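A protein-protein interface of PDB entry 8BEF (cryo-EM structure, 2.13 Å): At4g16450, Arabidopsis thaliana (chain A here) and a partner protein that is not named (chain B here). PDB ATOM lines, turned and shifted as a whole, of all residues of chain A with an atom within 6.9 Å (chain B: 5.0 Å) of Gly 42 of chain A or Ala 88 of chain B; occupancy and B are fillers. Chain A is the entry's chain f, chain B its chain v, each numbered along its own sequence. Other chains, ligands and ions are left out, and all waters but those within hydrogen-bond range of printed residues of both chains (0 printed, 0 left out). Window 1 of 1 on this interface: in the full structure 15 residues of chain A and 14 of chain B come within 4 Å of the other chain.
The backbone carbonyl oxygen (O) of Gly 42 of chain A lies within hydrogen-bond range of the side-chain hydroxyl (OG1) of Thr 46 of chain A.
Ala 88 of chain B touches just these residues of chain A: Gly 42 (3.8 Å), Val 45 (3.5 Å) and Thr 46 (3.8 Å). Of the printed residues of chain A, Gly 89 of chain B touches Thr 46. Of the printed residues of chain B, Met 62 of chain A touches Ala 85. Of the printed residues of chain B, Thr 46 of chain A touches Ala 88 (3.8 Å) and Gly 89 (3.4 Å). Of the printed residues of chain A, Ala 85 of chain B touches Met 62 (3.9 Å). Printed residues of chain A within 4 Å of Val 91 of chain B: Ser 38 (3.9 Å). The nearest printed residue of chain B that does not touch Gly 42 of chain A is Gly 89 of chain B (4.8 Å). The nearest residue of chain A that does not touch Ala 88 of chain B is Ile 43 of chain A (4.9 Å). The nearest printed residue of chain A that does not touch Gly 89 of chain B is Gly 42 of chain A (4.8 Å).
Hydrophobic or aromatic side chains of chain A within 4 Å of the printed part of chain B: Ile 43, Val 45 and Met 62. Along chain A the printed residues that touch a printed residue of chain B span positions 38 to 62. Among the printed residues, no Asp or Glu carboxylate lies within 4 Å of a Lys or Arg side-chain nitrogen of the other chain.
The side-chain hydroxyl (OG1) of Thr 46 of chain A sits at hydrogen-bond distance from the backbone NH (N) of Gly 89 of chain B.
Among the printed residues, pairs that only touch across the chains: Val 45 of chain A with Ala 88 of chain B (3.5 Å), Gly 42 of chain A with Ala 88 of chain B (3.8 Å), Thr 46 of chain A with Ala 88 of chain B (3.8 Å), Ile 43 of chain A with Ala 92 of chain B (3.8 Å), Met 62 of chain A with Ala 85 of chain B (3.9 Å), Ser 38 of chain A with Val 91 of chain B (3.9 Å) and Gly 42 of chain A with Ala 92 of chain B (3.96 Å).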
ATOM      1  N   ARG A  36      -3.555  15.515   8.988  1.00  0.00           N
ATOM      2  CA  ARG A  36      -4.843  15.614   8.304  1.00  0.00           C
ATOM      3  C   ARG A  36      -4.746  15.056   6.889  1.00  0.00           C
ATOM      4  O   ARG A  36      -5.597  14.270   6.447  1.00  0.00           O
ATOM      5  CB  ARG A  36      -5.306  17.072   8.252  1.00  0.00           C
ATOM      6  CG  ARG A  36      -5.640  17.720   9.584  1.00  0.00           C
ATOM      7  CD  ARG A  36      -5.565  19.238   9.449  1.00  0.00           C
ATOM      8  NE  ARG A  36      -6.070  19.940  10.622  1.00  0.00           N
ATOM      9  CZ  ARG A  36      -5.513  21.024  11.145  1.00  0.00           C
ATOM     10  NH1 ARG A  36      -4.419  21.558  10.627  1.00  0.00           N
ATOM     11  NH2 ARG A  36      -6.065  21.585  12.215  1.00  0.00           N
ATOM     12  N   PHE A  37      -3.703  15.473   6.168  1.00  0.00           N
ATOM     13  CA  PHE A  37      -3.452  15.030   4.803  1.00  0.00           C
ATOM     14  C   PHE A  37      -3.383  13.507   4.720  1.00  0.00           C
ATOM     15  O   PHE A  37      -4.104  12.871   3.937  1.00  0.00           O
ATOM     16  CB  PHE A  37      -2.139  15.678   4.345  1.00  0.00           C
ATOM     17  CG  PHE A  37      -1.889  15.635   2.869  1.00  0.00           C
ATOM     18  CD1 PHE A  37      -2.809  15.095   1.994  1.00  0.00           C
ATOM     19  CD2 PHE A  37      -0.714  16.164   2.356  1.00  0.00           C
ATOM     20  CE1 PHE A  37      -2.555  15.066   0.641  1.00  0.00           C
ATOM     21  CE2 PHE A  37      -0.461  16.139   1.007  1.00  0.00           C
ATOM     22  CZ  PHE A  37      -1.385  15.587   0.148  1.00  0.00           C
ATOM     23  N   SER A  38      -2.535  12.911   5.559  1.00  0.00           N
ATOM     24  CA  SER A  38      -2.316  11.472   5.524  1.00  0.00           C
ATOM     25  C   SER A  38      -3.568  10.711   5.936  1.00  0.00           C
ATOM     26  O   SER A  38      -3.883   9.675   5.345  1.00  0.00           O
ATOM     27  CB  SER A  38      -1.139  11.103   6.424  1.00  0.00           C
ATOM     28  OG  SER A  38      -1.528  11.114   7.784  1.00  0.00           O
ATOM     29  N   THR A  39      -4.294  11.203   6.943  1.00  0.00           N
ATOM     30  CA  THR A  39      -5.514  10.530   7.375  1.00  0.00           C
ATOM     31  C   THR A  39      -6.555  10.514   6.265  1.00  0.00           C
ATOM     32  O   THR A  39      -7.175   9.476   5.994  1.00  0.00           O
ATOM     33  CB  THR A  39      -6.080  11.210   8.624  1.00  0.00           C
ATOM     34  OG1 THR A  39      -5.134  11.120   9.695  1.00  0.00           O
ATOM     35  CG2 THR A  39      -7.387  10.556   9.047  1.00  0.00           C
ATOM     36  N   ILE A  40      -6.768  11.661   5.616  1.00  0.00           N
ATOM     37  CA  ILE A  40      -7.772  11.726   4.559  1.00  0.00           C
ATOM     38  C   ILE A  40      -7.387  10.800   3.412  1.00  0.00           C
ATOM     39  O   ILE A  40      -8.216  10.026   2.910  1.00  0.00           O
ATOM     40  CB  ILE A  40      -7.965  13.184   4.099  1.00  0.00           C
ATOM     41  CG1 ILE A  40      -8.782  13.955   5.141  1.00  0.00           C
ATOM     42  CG2 ILE A  40      -8.666  13.245   2.749  1.00  0.00           C
ATOM     43  CD1 ILE A  40      -8.524  15.442   5.150  1.00  0.00           C
ATOM     44  N   THR A  41      -6.110  10.823   3.014  1.00  0.00           N
ATOM     45  CA  THR A  41      -5.662   9.940   1.940  1.00  0.00           C
ATOM     46  C   THR A  41      -5.811   8.467   2.311  1.00  0.00           C
ATOM     47  O   THR A  41      -6.245   7.655   1.483  1.00  0.00           O
ATOM     48  CB  THR A  41      -4.214  10.259   1.572  1.00  0.00           C
ATOM     49  OG1 THR A  41      -4.071  11.672   1.378  1.00  0.00           O
ATOM     50  CG2 THR A  41      -3.804   9.511   0.310  1.00  0.00           C
ATOM     51  N   GLY A  42      -5.450   8.099   3.542  1.00  0.00           N
ATOM     52  CA  GLY A  42      -5.540   6.705   3.946  1.00  0.00           C
ATOM     53  C   GLY A  42      -6.968   6.199   3.994  1.00  0.00           C
ATOM     54  O   GLY A  42      -7.260   5.093   3.527  1.00  0.00           O
ATOM     55  N   ILE A  43      -7.876   7.001   4.555  1.00  0.00           N
ATOM     56  CA  ILE A  43      -9.288   6.633   4.559  1.00  0.00           C
ATOM     57  C   ILE A  43      -9.793   6.461   3.133  1.00  0.00           C
ATOM     58  O   ILE A  43     -10.540   5.521   2.830  1.00  0.00           O
ATOM     59  CB  ILE A  43     -10.113   7.683   5.327  1.00  0.00           C
ATOM     60  CG1 ILE A  43      -9.822   7.612   6.827  1.00  0.00           C
ATOM     61  CG2 ILE A  43     -11.603   7.500   5.067  1.00  0.00           C
ATOM     62  CD1 ILE A  43     -10.330   8.813   7.585  1.00  0.00           C
ATOM     63  N   SER A  44      -9.400   7.369   2.237  1.00  0.00           N
ATOM     64  CA  SER A  44      -9.874   7.285   0.861  1.00  0.00           C
ATOM     65  C   SER A  44      -9.363   6.027   0.165  1.00  0.00           C
ATOM     66  O   SER A  44     -10.116   5.363  -0.556  1.00  0.00           O
ATOM     67  CB  SER A  44      -9.464   8.540   0.100  1.00  0.00           C
ATOM     68  OG  SER A  44     -10.161   9.671   0.591  1.00  0.00           O
ATOM     69  N   VAL A  45      -8.090   5.679   0.379  1.00  0.00           N
ATOM     70  CA  VAL A  45      -7.548   4.454  -0.206  1.00  0.00           C
ATOM     71  C   VAL A  45      -8.279   3.233   0.342  1.00  0.00           C
ATOM     72  O   VAL A  45      -8.584   2.288  -0.396  1.00  0.00           O
ATOM     73  CB  VAL A  45      -6.030   4.358   0.038  1.00  0.00           C
ATOM     74  CG1 VAL A  45      -5.505   3.003  -0.412  1.00  0.00           C
ATOM     75  CG2 VAL A  45      -5.296   5.472  -0.685  1.00  0.00           C
ATOM     76  N   THR A  46      -8.560   3.230   1.649  1.00  0.00           N
ATOM     77  CA  THR A  46      -9.267   2.108   2.258  1.00  0.00           C
ATOM     78  C   THR A  46     -10.661   1.942   1.659  1.00  0.00           C
ATOM     79  O   THR A  46     -11.088   0.823   1.346  1.00  0.00           O
ATOM     80  CB  THR A  46      -9.351   2.311   3.773  1.00  0.00           C
ATOM     81  OG1 THR A  46      -8.040   2.209   4.343  1.00  0.00           O
ATOM     82  CG2 THR A  46     -10.262   1.269   4.409  1.00  0.00           C
ATOM     83  N   VAL A  47     -11.386   3.053   1.500  1.00  0.00           N
ATOM     84  CA  VAL A  47     -12.717   2.996   0.902  1.00  0.00           C
ATOM     85  C   VAL A  47     -12.630   2.491  -0.532  1.00  0.00           C
ATOM     86  O   VAL A  47     -13.440   1.662  -0.962  1.00  0.00           O
ATOM     87  CB  VAL A  47     -13.410   4.371   0.985  1.00  0.00           C
ATOM     88  CG1 VAL A  47     -14.708   4.367   0.189  1.00  0.00           C
ATOM     89  CG2 VAL A  47     -13.688   4.743   2.434  1.00  0.00           C
ATOM     90  N   GLY A  48     -11.639   2.973  -1.287  1.00  0.00           N
ATOM     91  CA  GLY A  48     -11.455   2.478  -2.641  1.00  0.00           C
ATOM     92  C   GLY A  48     -11.240   0.978  -2.685  1.00  0.00           C
ATOM     93  O   GLY A  48     -11.876   0.272  -3.467  1.00  0.00           O
ATOM     94  N   MET A  62      -8.593   1.335  -5.504  1.00  0.00           N
ATOM     95  CA  MET A  62      -7.691   1.941  -4.534  1.00  0.00           C
ATOM     96  C   MET A  62      -7.002   3.157  -5.122  1.00  0.00           C
ATOM     97  O   MET A  62      -6.855   4.179  -4.448  1.00  0.00           O
ATOM     98  CB  MET A  62      -6.642   0.931  -4.078  1.00  0.00           C
ATOM     99  CG  MET A  62      -6.812   0.446  -2.671  1.00  0.00           C
ATOM    100  SD  MET A  62      -5.291  -0.295  -2.047  1.00  0.00           S
ATOM    101  CE  MET A  62      -5.088  -1.615  -3.231  1.00  0.00           C
ATOM    102  N   GLY A  69      -8.593  11.207  -2.419  1.00  0.00           N
ATOM    103  CA  GLY A  69      -8.120  11.540  -1.089  1.00  0.00           C
ATOM    104  C   GLY A  69      -6.903  12.443  -1.095  1.00  0.00           C
ATOM    105  O   GLY A  69      -6.785  13.331  -0.256  1.00  0.00           O
ATOM    106  N   TYR B  84      -1.091  -3.268   0.550  1.00  0.00           N
ATOM    107  CA  TYR B  84      -1.153  -1.814   0.443  1.00  0.00           C
ATOM    108  C   TYR B  84      -2.388  -1.269   1.148  1.00  0.00           C
ATOM    109  O   TYR B  84      -2.319  -0.247   1.840  1.00  0.00           O
ATOM    110  CB  TYR B  84      -1.143  -1.393  -1.028  1.00  0.00           C
ATOM    111  CG  TYR B  84       0.103  -1.798  -1.783  1.00  0.00           C
ATOM    112  CD1 TYR B  84       1.288  -2.074  -1.115  1.00  0.00           C
ATOM    113  CD2 TYR B  84       0.087  -1.921  -3.164  1.00  0.00           C
ATOM    114  CE1 TYR B  84       2.420  -2.449  -1.801  1.00  0.00           C
ATOM    115  CE2 TYR B  84       1.214  -2.296  -3.860  1.00  0.00           C
ATOM    116  CZ  TYR B  84       2.379  -2.560  -3.175  1.00  0.00           C
ATOM    117  OH  TYR B  84       3.504  -2.938  -3.864  1.00  0.00           O
ATOM    118  N   ALA B  85      -3.529  -1.945   0.987  1.00  0.00           N
ATOM    119  CA  ALA B  85      -4.744  -1.524   1.679  1.00  0.00           C
ATOM    120  C   ALA B  85      -4.579  -1.618   3.190  1.00  0.00           C
ATOM    121  O   ALA B  85      -5.083  -0.769   3.935  1.00  0.00           O
ATOM    122  CB  ALA B  85      -5.930  -2.367   1.216  1.00  0.00           C
ATOM    123  N   VAL B  86      -3.885  -2.654   3.660  1.00  0.00           N
ATOM    124  CA  VAL B  86      -3.609  -2.785   5.087  1.00  0.00           C
ATOM    125  C   VAL B  86      -2.773  -1.608   5.574  1.00  0.00           C
ATOM    126  O   VAL B  86      -3.054  -1.017   6.626  1.00  0.00           O
ATOM    127  CB  VAL B  86      -2.920  -4.133   5.370  1.00  0.00           C
ATOM    128  CG1 VAL B  86      -2.317  -4.143   6.751  1.00  0.00           C
ATOM    129  CG2 VAL B  86      -3.910  -5.271   5.209  1.00  0.00           C
ATOM    130  N   VAL B  87      -1.742  -1.244   4.810  1.00  0.00           N
ATOM    131  CA  VAL B  87      -0.921  -0.090   5.172  1.00  0.00           C
ATOM    132  C   VAL B  87      -1.768   1.176   5.208  1.00  0.00           C
ATOM    133  O   VAL B  87      -1.615   2.015   6.102  1.00  0.00           O
ATOM    134  CB  VAL B  87       0.271   0.055   4.208  1.00  0.00           C
ATOM    135  CG1 VAL B  87       1.029   1.348   4.490  1.00  0.00           C
ATOM    136  CG2 VAL B  87       1.202  -1.135   4.333  1.00  0.00           C
ATOM    137  N   ALA B  88      -2.665   1.339   4.235  1.00  0.00           N
ATOM    138  CA  ALA B  88      -3.514   2.528   4.191  1.00  0.00           C
ATOM    139  C   ALA B  88      -4.438   2.603   5.400  1.00  0.00           C
ATOM    140  O   ALA B  88      -4.625   3.678   5.981  1.00  0.00           O
ATOM    141  CB  ALA B  88      -4.328   2.550   2.900  1.00  0.00           C
ATOM    142  N   GLY B  89      -5.036   1.476   5.785  1.00  0.00           N
ATOM    143  CA  GLY B  89      -5.874   1.467   6.973  1.00  0.00           C
ATOM    144  C   GLY B  89      -5.094   1.784   8.236  1.00  0.00           C
ATOM    145  O   GLY B  89      -5.563   2.531   9.102  1.00  0.00           O
ATOM    146  N   VAL B  90      -3.885   1.230   8.352  1.00  0.00           N
ATOM    147  CA  VAL B  90      -3.046   1.515   9.513  1.00  0.00           C
ATOM    148  C   VAL B  90      -2.676   2.992   9.550  1.00  0.00           C
ATOM    149  O   VAL B  90      -2.701   3.628  10.611  1.00  0.00           O
ATOM    150  CB  VAL B  90      -1.793   0.617   9.500  1.00  0.00           C
ATOM    151  CG1 VAL B  90      -0.723   1.184  10.416  1.00  0.00           C
ATOM    152  CG2 VAL B  90      -2.153  -0.804   9.902  1.00  0.00           C
ATOM    153  N   VAL B  91      -2.318   3.555   8.395  1.00  0.00           N
ATOM    154  CA  VAL B  91      -1.976   4.971   8.324  1.00  0.00           C
ATOM    155  C   VAL B  91      -3.174   5.822   8.715  1.00  0.00           C
ATOM    156  O   VAL B  91      -3.035   6.805   9.444  1.00  0.00           O
ATOM    157  CB  VAL B  91      -1.452   5.329   6.919  1.00  0.00           C
ATOM    158  CG1 VAL B  91      -1.542   6.832   6.665  1.00  0.00           C
ATOM    159  CG2 VAL B  91      -0.017   4.852   6.749  1.00  0.00           C
ATOM    160  N   ALA B  92      -4.370   5.445   8.260  1.00  0.00           N
ATOM    161  CA  ALA B  92      -5.569   6.188   8.637  1.00  0.00           C
ATOM    162  C   ALA B  92      -5.780   6.162  10.147  1.00  0.00           C
ATOM    163  O   ALA B  92      -6.028   7.201  10.767  1.00  0.00           O
ATOM    164  CB  ALA B  92      -6.791   5.623   7.912  1.00  0.00           C
